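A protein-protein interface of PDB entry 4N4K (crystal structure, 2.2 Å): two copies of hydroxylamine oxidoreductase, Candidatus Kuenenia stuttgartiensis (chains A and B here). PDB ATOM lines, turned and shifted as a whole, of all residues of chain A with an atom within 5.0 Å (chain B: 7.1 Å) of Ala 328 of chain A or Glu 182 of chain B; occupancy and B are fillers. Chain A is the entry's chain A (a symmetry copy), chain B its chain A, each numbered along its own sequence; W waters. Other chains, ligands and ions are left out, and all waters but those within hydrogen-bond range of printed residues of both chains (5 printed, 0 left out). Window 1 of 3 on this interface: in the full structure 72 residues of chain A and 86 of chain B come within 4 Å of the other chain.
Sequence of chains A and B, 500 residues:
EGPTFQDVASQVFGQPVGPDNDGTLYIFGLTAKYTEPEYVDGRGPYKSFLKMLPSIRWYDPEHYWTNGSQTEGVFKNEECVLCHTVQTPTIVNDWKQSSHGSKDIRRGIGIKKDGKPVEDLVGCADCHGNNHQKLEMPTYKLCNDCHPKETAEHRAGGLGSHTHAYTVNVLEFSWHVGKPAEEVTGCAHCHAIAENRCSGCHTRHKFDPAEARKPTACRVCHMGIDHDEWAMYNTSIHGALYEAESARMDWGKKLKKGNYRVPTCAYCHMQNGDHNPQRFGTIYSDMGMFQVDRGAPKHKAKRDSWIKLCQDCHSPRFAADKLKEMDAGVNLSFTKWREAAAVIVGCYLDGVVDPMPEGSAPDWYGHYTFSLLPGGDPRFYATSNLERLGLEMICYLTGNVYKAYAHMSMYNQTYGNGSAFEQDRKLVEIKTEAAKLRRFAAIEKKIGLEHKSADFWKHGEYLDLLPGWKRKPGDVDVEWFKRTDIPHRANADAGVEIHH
OE1 of Glu 183 of chain B lies within salt-bridge range of NZ of Lys 179 of chain B, at 2.6 Å.
OG1 of Thr 35 of chain B sits at hydrogen-bond distance from OD2 of Asp 20 of chain B (2.7 Å).
OH of Tyr 34 of chain B sits at hydrogen-bond distance from OE1 of Glu 182 of chain B, at 2.7 Å.
The side-chain hydroxyl (OH) of Tyr 39 of chain B sits at hydrogen-bond distance from the side-chain carboxylate (OE2) of Glu 182 of chain B (2.6 Å).
The backbone carbonyl oxygen (O) of Asp 327 of chain A sits close to the side-chain amide nitrogen (ND2) of Asn 331 of chain A (3.4 Å).
Among the printed residues, merely in contact across the chains: Asn 331 of chain A with Asp 20 of chain B (3.4 Å), Ala 328 of chain A with Glu 182 of chain B (3.5 Å), Leu 332 of chain A with Glu 182 of chain B (3.7 Å), Glu 325 of chain A with Thr 185 of chain B (3.7 Å), Leu 332 of chain A with Glu 183 of chain B (3.9 Å), Gly 329 of chain A with Glu 182 of chain B (3.9 Å), Tyr 405 of chain A with Glu 183 of chain B (3.9 Å) and Leu 332 of chain A with Tyr 34 of chain B (3.997 Å).
Water W4 lies within hydrogen-bond range of OH of Tyr 405 of chain A (2.6 Å) and O of Glu 183 of chain B (2.7 Å).
Water W1 bridges OD1 of Asp 20 of chain B (2.6 Å) and O of Asn 331 of chain A (2.7 Å).
Water W2 lies within hydrogen-bond range of O of Glu 182 of chain B (2.7 Å), OG1 of Thr 185 of chain B (2.7 Å) and O of Glu 325 of chain A (3.0 Å).
Water W3 lies within hydrogen-bond range of O of Ala 328 of chain A and OE1 of Glu 182 of chain B.
Water W5 lies within hydrogen-bond range of OH of Tyr 405 of chain A (2.8 Å) and N of Gly 186 of chain B (2.8 Å).
Glu 182 of chain B touches four residues of chain A.
Printed residues of chain B within 4 Å of Asn 331 of chain A: Asp 20 (3.4 Å).
Printed residues of chain A within 4 Å of Tyr 34 of chain B: Leu 332.
Printed residues of chain B within 4 Å of Leu 332 of chain A: Tyr 34 (3.997 Å), Glu 182 (3.7 Å) and Glu 183 (3.9 Å).
Printed residues of chain B within 4 Å of Tyr 405 of chain A: Glu 182 (3.0 Å) and Glu 183 (3.9 Å).
Tyr 39 of chain B touches none of the printed residues of chain A.
Val 184 of chain B touches none of the printed residues of chain A.
The nearest printed residue of chain A that does not touch Glu 182 of chain B is Glu 325 of chain A (5.1 Å).
The backbone carbonyl oxygen (O) of Glu 182 of chain B is in hydrogen-bond range of the side-chain hydroxyl (OH) of Tyr 405 of chain A (3.0 Å).
Hydrophobic or aromatic side chains of chain A that line the printed part of chain B: Ala 328, Leu 332 and Tyr 405.
Of the 18 printed residues of chain B, 5 touch a printed residue of chain A.
Hydrophobic or aromatic side chains of chain B within 4 Å of the printed part of chain A: Tyr 34.
Along chain B the printed residues that touch a printed residue of chain A span positions 20 to 185.
Among the printed residues, 9 pairs touch across the chains.
No position is printed for both chains.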
ATOM      1  N   LYS A 324       2.520 -16.808  26.051  1.00  0.00           N
ATOM      2  CA  LYS A 324       2.316 -15.394  26.429  1.00  0.00           C
ATOM      3  C   LYS A 324       0.829 -15.019  26.428  1.00  0.00           C
ATOM      4  O   LYS A 324       0.401 -14.169  27.210  1.00  0.00           O
ATOM      5  CB  LYS A 324       3.083 -14.446  25.495  1.00  0.00           C
ATOM      6  CG  LYS A 324       4.562 -14.293  25.812  1.00  0.00           C
ATOM      7  CD  LYS A 324       5.275 -13.576  24.665  1.00  0.00           C
ATOM      8  CE  LYS A 324       6.763 -13.383  24.932  1.00  0.00           C
ATOM      9  NZ  LYS A 324       7.490 -13.020  23.670  1.00  0.00           N
ATOM     10  N   GLU A 325       0.066 -15.598  25.503  1.00  0.00           N
ATOM     11  CA  GLU A 325      -1.386 -15.412  25.474  1.00  0.00           C
ATOM     12  C   GLU A 325      -2.018 -15.935  26.753  1.00  0.00           C
ATOM     13  O   GLU A 325      -3.019 -15.389  27.220  1.00  0.00           O
ATOM     14  CB  GLU A 325      -2.007 -16.132  24.275  1.00  0.00           C
ATOM     15  CG  GLU A 325      -1.678 -15.493  22.944  1.00  0.00           C
ATOM     16  CD  GLU A 325      -2.024 -16.380  21.770  1.00  0.00           C
ATOM     17  OE1 GLU A 325      -2.765 -17.365  21.953  1.00  0.00           O
ATOM     18  OE2 GLU A 325      -1.595 -16.059  20.646  1.00  0.00           O
ATOM     19  N   MET A 326      -1.508 -17.065  27.237  1.00  0.00           N
ATOM     20  CA  MET A 326      -1.943 -17.625  28.518  1.00  0.00           C
ATOM     21  C   MET A 326      -1.694 -16.637  29.648  1.00  0.00           C
ATOM     22  O   MET A 326      -2.607 -16.324  30.411  1.00  0.00           O
ATOM     23  CB  MET A 326      -1.219 -18.947  28.807  1.00  0.00           C
ATOM     24  CG  MET A 326      -1.473 -19.528  30.197  1.00  0.00           C
ATOM     25  SD  MET A 326      -0.581 -21.069  30.494  1.00  0.00           S
ATOM     26  CE  MET A 326       1.119 -20.490  30.460  1.00  0.00           C
ATOM     27  N   ASP A 327      -0.492 -16.069  29.683  1.00  0.00           N
ATOM     28  CA  ASP A 327      -0.120 -15.126  30.745  1.00  0.00           C
ATOM     29  C   ASP A 327      -1.052 -13.918  30.735  1.00  0.00           C
ATOM     30  O   ASP A 327      -1.686 -13.606  31.747  1.00  0.00           O
ATOM     31  CB  ASP A 327       1.329 -14.645  30.583  1.00  0.00           C
ATOM     32  CG  ASP A 327       2.339 -15.779  30.599  1.00  0.00           C
ATOM     33  OD1 ASP A 327       2.106 -16.799  31.294  1.00  0.00           O
ATOM     34  OD2 ASP A 327       3.407 -15.615  29.972  1.00  0.00           O
ATOM     35  N   ALA A 328      -1.261 -13.355  29.547  1.00  0.00           N
ATOM     36  CA  ALA A 328      -2.129 -12.183  29.388  1.00  0.00           C
ATOM     37  C   ALA A 328      -3.597 -12.496  29.718  1.00  0.00           C
ATOM     38  O   ALA A 328      -4.250 -11.749  30.447  1.00  0.00           O
ATOM     39  CB  ALA A 328      -2.008 -11.622  27.972  1.00  0.00           C
ATOM     40  N   GLY A 329      -4.077 -13.647  29.256  1.00  0.00           N
ATOM     41  CA  GLY A 329      -5.460 -14.055  29.494  1.00  0.00           C
ATOM     42  C   GLY A 329      -5.739 -14.347  30.954  1.00  0.00           C
ATOM     43  O   GLY A 329      -6.808 -14.017  31.469  1.00  0.00           O
ATOM     44  N   VAL A 330      -4.767 -14.953  31.630  1.00  0.00           N
ATOM     45  CA  VAL A 330      -4.892 -15.239  33.056  1.00  0.00           C
ATOM     46  C   VAL A 330      -4.904 -13.940  33.877  1.00  0.00           C
ATOM     47  O   VAL A 330      -5.832 -13.706  34.647  1.00  0.00           O
ATOM     48  CB  VAL A 330      -3.762 -16.190  33.540  1.00  0.00           C
ATOM     49  CG1 VAL A 330      -3.666 -16.194  35.057  1.00  0.00           C
ATOM     50  CG2 VAL A 330      -3.997 -17.604  33.006  1.00  0.00           C
ATOM     51  N   ASN A 331      -4.025 -13.004  33.521  1.00  0.00           N
ATOM     52  CA  ASN A 331      -3.940 -11.727  34.238  1.00  0.00           C
ATOM     53  C   ASN A 331      -5.195 -10.868  34.074  1.00  0.00           C
ATOM     54  O   ASN A 331      -5.698 -10.322  35.061  1.00  0.00           O
ATOM     55  CB  ASN A 331      -2.689 -10.943  33.817  1.00  0.00           C
ATOM     56  CG  ASN A 331      -1.402 -11.559  34.356  1.00  0.00           C
ATOM     57  OD1 ASN A 331      -1.429 -12.377  35.276  1.00  0.00           O
ATOM     58  ND2 ASN A 331      -0.286 -11.243  33.719  1.00  0.00           N
ATOM     59  N   LEU A 332      -5.826 -10.950  32.906  1.00  0.00           N
ATOM     60  CA  LEU A 332      -7.101 -10.263  32.683  1.00  0.00           C
ATOM     61  C   LEU A 332      -8.206 -10.892  33.520  1.00  0.00           C
ATOM     62  O   LEU A 332      -8.994 -10.175  34.140  1.00  0.00           O
ATOM     63  CB  LEU A 332      -7.494 -10.295  31.202  1.00  0.00           C
ATOM     64  CG  LEU A 332      -8.727  -9.487  30.745  1.00  0.00           C
ATOM     65  CD1 LEU A 332     -10.047 -10.096  31.210  1.00  0.00           C
ATOM     66  CD2 LEU A 332      -8.630  -8.027  31.181  1.00  0.00           C
ATOM     67  N   TYR A 405      -6.356 -21.746  28.599  1.00  0.00           N
ATOM     68  CA  TYR A 405      -5.209 -21.186  27.890  1.00  0.00           C
ATOM     69  C   TYR A 405      -4.040 -22.167  27.800  1.00  0.00           C
ATOM     70  O   TYR A 405      -3.439 -22.310  26.736  1.00  0.00           O
ATOM     71  CB  TYR A 405      -4.748 -19.878  28.534  1.00  0.00           C
ATOM     72  CG  TYR A 405      -5.536 -18.665  28.077  1.00  0.00           C
ATOM     73  CD1 TYR A 405      -6.566 -18.140  28.853  1.00  0.00           C
ATOM     74  CD2 TYR A 405      -5.253 -18.046  26.861  1.00  0.00           C
ATOM     75  CE1 TYR A 405      -7.273 -17.019  28.439  1.00  0.00           C
ATOM     76  CE2 TYR A 405      -6.006 -16.981  26.406  1.00  0.00           C
ATOM     77  CZ  TYR A 405      -6.999 -16.457  27.203  1.00  0.00           C
ATOM     78  OH  TYR A 405      -7.728 -15.381  26.758  1.00  0.00           O
ATOM     79  N   ASP B  20       0.912  -7.611  38.427  1.00  0.00           N
ATOM     80  CA  ASP B  20       0.557  -8.998  38.120  1.00  0.00           C
ATOM     81  C   ASP B  20       1.627  -9.735  37.312  1.00  0.00           C
ATOM     82  O   ASP B  20       1.821 -10.933  37.510  1.00  0.00           O
ATOM     83  CB  ASP B  20      -0.799  -9.079  37.398  1.00  0.00           C
ATOM     84  CG  ASP B  20      -0.853  -8.254  36.113  1.00  0.00           C
ATOM     85  OD1 ASP B  20      -1.966  -8.097  35.566  1.00  0.00           O
ATOM     86  OD2 ASP B  20       0.191  -7.757  35.647  1.00  0.00           O
ATOM     87  N   TYR B  34      -3.405  -5.031  37.983  1.00  0.00           N
ATOM     88  CA  TYR B  34      -3.475  -5.263  36.546  1.00  0.00           C
ATOM     89  C   TYR B  34      -2.502  -4.358  35.798  1.00  0.00           C
ATOM     90  O   TYR B  34      -2.484  -3.147  36.019  1.00  0.00           O
ATOM     91  CB  TYR B  34      -4.893  -5.020  36.028  1.00  0.00           C
ATOM     92  CG  TYR B  34      -5.004  -5.059  34.519  1.00  0.00           C
ATOM     93  CD1 TYR B  34      -5.087  -6.272  33.842  1.00  0.00           C
ATOM     94  CD2 TYR B  34      -4.994  -3.883  33.768  1.00  0.00           C
ATOM     95  CE1 TYR B  34      -5.254  -6.315  32.466  1.00  0.00           C
ATOM     96  CE2 TYR B  34      -5.132  -3.915  32.385  1.00  0.00           C
ATOM     97  CZ  TYR B  34      -5.262  -5.136  31.741  1.00  0.00           C
ATOM     98  OH  TYR B  34      -5.381  -5.184  30.375  1.00  0.00           O
ATOM     99  N   THR B  35      -1.693  -4.962  34.930  1.00  0.00           N
ATOM    100  CA  THR B  35      -0.866  -4.224  33.980  1.00  0.00           C
ATOM    101  C   THR B  35      -1.406  -4.452  32.571  1.00  0.00           C
ATOM    102  O   THR B  35      -1.842  -5.555  32.234  1.00  0.00           O
ATOM    103  CB  THR B  35       0.593  -4.693  34.004  1.00  0.00           C
ATOM    104  OG1 THR B  35       0.664  -6.070  33.608  1.00  0.00           O
ATOM    105  CG2 THR B  35       1.189  -4.522  35.400  1.00  0.00           C
ATOM    106  N   GLU B  36      -1.211  -3.462  31.709  1.00  0.00           N
ATOM    107  CA  GLU B  36      -1.670  -3.551  30.333  1.00  0.00           C
ATOM    108  C   GLU B  36      -0.627  -4.286  29.509  1.00  0.00           C
ATOM    109  O   GLU B  36       0.528  -3.869  29.475  1.00  0.00           O
ATOM    110  CB  GLU B  36      -1.901  -2.157  29.748  1.00  0.00           C
ATOM    111  CG  GLU B  36      -2.882  -2.149  28.593  1.00  0.00           C
ATOM    112  CD  GLU B  36      -3.041  -0.774  27.971  1.00  0.00           C
ATOM    113  OE1 GLU B  36      -4.010  -0.085  28.342  1.00  0.00           O
ATOM    114  OE2 GLU B  36      -2.094  -0.312  27.299  1.00  0.00           O
ATOM    115  N   PRO B  37      -1.008  -5.418  28.890  1.00  0.00           N
ATOM    116  CA  PRO B  37      -0.061  -6.094  28.004  1.00  0.00           C
ATOM    117  C   PRO B  37       0.344  -5.236  26.811  1.00  0.00           C
ATOM    118  O   PRO B  37      -0.372  -4.299  26.448  1.00  0.00           O
ATOM    119  CB  PRO B  37      -0.833  -7.329  27.511  1.00  0.00           C
ATOM    120  CG  PRO B  37      -2.152  -7.309  28.172  1.00  0.00           C
ATOM    121  CD  PRO B  37      -2.365  -5.979  28.789  1.00  0.00           C
ATOM    122  N   TYR B  39       0.405  -4.269  23.206  1.00  0.00           N
ATOM    123  CA  TYR B  39      -0.541  -4.467  22.114  1.00  0.00           C
ATOM    124  C   TYR B  39       0.029  -3.988  20.784  1.00  0.00           C
ATOM    125  O   TYR B  39       1.016  -3.250  20.739  1.00  0.00           O
ATOM    126  CB  TYR B  39      -1.837  -3.691  22.371  1.00  0.00           C
ATOM    127  CG  TYR B  39      -2.573  -4.036  23.652  1.00  0.00           C
ATOM    128  CD1 TYR B  39      -3.026  -5.334  23.875  1.00  0.00           C
ATOM    129  CD2 TYR B  39      -3.117  -3.017  24.439  1.00  0.00           C
ATOM    130  CE1 TYR B  39      -3.872  -5.629  24.939  1.00  0.00           C
ATOM    131  CE2 TYR B  39      -4.017  -3.293  25.463  1.00  0.00           C
ATOM    132  CZ  TYR B  39      -4.344  -4.606  25.747  1.00  0.00           C
ATOM    133  OH  TYR B  39      -5.199  -4.886  26.792  1.00  0.00           O
ATOM    134  N   LYS B  51      -7.372  -3.117  19.738  1.00  0.00           N
ATOM    135  CA  LYS B  51      -6.033  -3.657  19.948  1.00  0.00           C
ATOM    136  C   LYS B  51      -6.054  -5.169  19.795  1.00  0.00           C
ATOM    137  O   LYS B  51      -7.128  -5.779  19.786  1.00  0.00           O
ATOM    138  CB  LYS B  51      -5.514  -3.298  21.345  1.00  0.00           C
ATOM    139  CG  LYS B  51      -5.523  -1.808  21.681  1.00  0.00           C
ATOM    140  CD  LYS B  51      -4.591  -1.009  20.777  1.00  0.00           C
ATOM    141  CE  LYS B  51      -4.560   0.476  21.163  1.00  0.00           C
ATOM    142  NZ  LYS B  51      -3.613   1.251  20.295  1.00  0.00           N
ATOM    143  N   MET B  52      -4.906  -5.699  19.382  1.00  0.00           N
ATOM    144  CA  MET B  52      -4.645  -7.133  19.349  1.00  0.00           C
ATOM    145  C   MET B  52      -3.364  -7.394  20.127  1.00  0.00           C
ATOM    146  O   MET B  52      -2.518  -6.506  20.234  1.00  0.00           O
ATOM    147  CB  MET B  52      -4.435  -7.596  17.904  1.00  0.00           C
ATOM    148  CG  MET B  52      -5.658  -7.477  17.023  1.00  0.00           C
ATOM    149  SD  MET B  52      -6.833  -8.795  17.344  1.00  0.00           S
ATOM    150  CE  MET B  52      -8.252  -8.207  16.429  1.00  0.00           C
ATOM    151  N   LEU B  53      -3.193  -8.619  20.618  1.00  0.00           N
ATOM    152  CA  LEU B  53      -1.888  -9.053  21.108  1.00  0.00           C
ATOM    153  C   LEU B  53      -0.992  -9.291  19.889  1.00  0.00           C
ATOM    154  O   LEU B  53      -1.500  -9.602  18.807  1.00  0.00           O
ATOM    155  CB  LEU B  53      -1.989 -10.325  21.951  1.00  0.00           C
ATOM    156  CG  LEU B  53      -2.724 -10.224  23.291  1.00  0.00           C
ATOM    157  CD1 LEU B  53      -2.756 -11.583  23.969  1.00  0.00           C
ATOM    158  CD2 LEU B  53      -2.091  -9.187  24.207  1.00  0.00           C
ATOM    159  N   LYS B 179     -14.213  -5.406  24.362  1.00  0.00           N
ATOM    160  CA  LYS B 179     -13.468  -6.056  25.443  1.00  0.00           C
ATOM    161  C   LYS B 179     -11.967  -5.876  25.269  1.00  0.00           C
ATOM    162  O   LYS B 179     -11.487  -5.746  24.142  1.00  0.00           O
ATOM    163  CB  LYS B 179     -13.812  -7.548  25.495  1.00  0.00           C
ATOM    164  CG  LYS B 179     -15.205  -7.834  26.048  1.00  0.00           C
ATOM    165  CD  LYS B 179     -15.537  -9.317  26.022  1.00  0.00           C
ATOM    166  CE  LYS B 179     -16.693  -9.647  26.940  1.00  0.00           C
ATOM    167  NZ  LYS B 179     -16.311  -9.529  28.377  1.00  0.00           N
ATOM    168  N   PRO B 180     -11.208  -5.925  26.378  1.00  0.00           N
ATOM    169  CA  PRO B 180      -9.749  -5.892  26.271  1.00  0.00           C
ATOM    170  C   PRO B 180      -9.229  -7.040  25.413  1.00  0.00           C
ATOM    171  O   PRO B 180      -9.803  -8.134  25.429  1.00  0.00           O
ATOM    172  CB  PRO B 180      -9.283  -6.045  27.719  1.00  0.00           C
ATOM    173  CG  PRO B 180     -10.410  -5.567  28.532  1.00  0.00           C
ATOM    174  CD  PRO B 180     -11.652  -5.925  27.782  1.00  0.00           C
ATOM    175  N   ALA B 181      -8.263  -6.723  24.555  1.00  0.00           N
ATOM    176  CA  ALA B 181      -7.794  -7.624  23.512  1.00  0.00           C
ATOM    177  C   ALA B 181      -7.452  -9.021  24.014  1.00  0.00           C
ATOM    178  O   ALA B 181      -7.791 -10.011  23.363  1.00  0.00           O
ATOM    179  CB  ALA B 181      -6.585  -7.016  22.803  1.00  0.00           C
ATOM    180  N   GLU B 182      -6.738  -9.099  25.137  1.00  0.00           N
ATOM    181  CA  GLU B 182      -6.249 -10.384  25.650  1.00  0.00           C
ATOM    182  C   GLU B 182      -7.376 -11.290  26.148  1.00  0.00           C
ATOM    183  O   GLU B 182      -7.158 -12.479  26.389  1.00  0.00           O
ATOM    184  CB  GLU B 182      -5.196 -10.186  26.750  1.00  0.00           C
ATOM    185  CG  GLU B 182      -5.727  -9.627  28.075  1.00  0.00           C
ATOM    186  CD  GLU B 182      -5.571  -8.126  28.219  1.00  0.00           C
ATOM    187  OE1 GLU B 182      -5.326  -7.672  29.358  1.00  0.00           O
ATOM    188  OE2 GLU B 182      -5.674  -7.401  27.204  1.00  0.00           O
ATOM    189  N   GLU B 183      -8.539 -10.697  26.414  1.00  0.00           N
ATOM    190  CA  GLU B 183      -9.712 -11.458  26.845  1.00  0.00           C
ATOM    191  C   GLU B 183     -10.333 -12.259  25.700  1.00  0.00           C
ATOM    192  O   GLU B 183     -10.936 -13.310  25.934  1.00  0.00           O
ATOM    193  CB  GLU B 183     -10.771 -10.529  27.451  1.00  0.00           C
ATOM    194  CG  GLU B 183     -12.011 -11.256  27.973  1.00  0.00           C
ATOM    195  CD  GLU B 183     -13.044 -10.327  28.574  1.00  0.00           C
ATOM    196  OE1 GLU B 183     -14.137 -10.820  28.929  1.00  0.00           O
ATOM    197  OE2 GLU B 183     -12.840  -9.097  28.519  1.00  0.00           O
ATOM    198  N   VAL B 184     -10.110 -11.806  24.469  1.00  0.00           N
ATOM    199  CA  VAL B 184     -10.779 -12.370  23.300  1.00  0.00           C
ATOM    200  C   VAL B 184      -9.797 -12.770  22.188  1.00  0.00           C
ATOM    201  O   VAL B 184     -10.193 -12.923  21.034  1.00  0.00           O
ATOM    202  CB  VAL B 184     -11.848 -11.377  22.766  1.00  0.00           C
ATOM    203  CG1 VAL B 184     -12.931 -11.146  23.833  1.00  0.00           C
ATOM    204  CG2 VAL B 184     -11.218 -10.055  22.369  1.00  0.00           C
ATOM    205  N   THR B 185      -8.581 -13.150  22.580  1.00  0.00           N
ATOM    206  CA  THR B 185      -7.572 -13.632  21.633  1.00  0.00           C
ATOM    207  C   THR B 185      -8.086 -14.844  20.844  1.00  0.00           C
ATOM    208  O   THR B 185      -8.050 -14.854  19.617  1.00  0.00           O
ATOM    209  CB  THR B 185      -6.267 -14.030  22.359  1.00  0.00           C
ATOM    210  OG1 THR B 185      -5.752 -12.905  23.088  1.00  0.00           O
ATOM    211  CG2 THR B 185      -5.221 -14.512  21.360  1.00  0.00           C
ATOM    212  N   GLY B 186      -8.713 -15.778  21.550  1.00  0.00           N
ATOM    213  CA  GLY B 186      -9.264 -16.979  20.926  1.00  0.00           C
ATOM    214  C   GLY B 186     -10.337 -16.705  19.885  1.00  0.00           C
ATOM    215  O   GLY B 186     -10.599 -17.552  19.036  1.00  0.00           O
ATOM    216  N   LEU B 465     -11.831  -0.941  32.477  1.00  0.00           N
ATOM    217  CA  LEU B 465     -10.993  -1.206  31.295  1.00  0.00           C
ATOM    218  C   LEU B 465     -11.759  -1.137  29.973  1.00  0.00           C
ATOM    219  O   LEU B 465     -11.142  -1.111  28.904  1.00  0.00           O
ATOM    220  CB  LEU B 465     -10.331  -2.584  31.402  1.00  0.00           C
ATOM    221  CG  LEU B 465      -9.329  -2.792  32.536  1.00  0.00           C
ATOM    222  CD1 LEU B 465      -8.880  -4.255  32.581  1.00  0.00           C
ATOM    223  CD2 LEU B 465      -8.128  -1.850  32.388  1.00  0.00           C
HETATM  224  O   HOH W   1      -4.100  -9.027  36.768  1.00  0.00           O
HETATM  225  O   HOH W   2      -4.854 -13.618  25.581  1.00  0.00           O
HETATM  226  O   HOH W   3      -3.564  -9.157  30.856  1.00  0.00           O
HETATM  227  O   HOH W   4     -10.089 -15.053  27.838  1.00  0.00           O
HETATM  228  O   HOH W   5      -8.763 -16.276  24.316  1.00  0.00           O
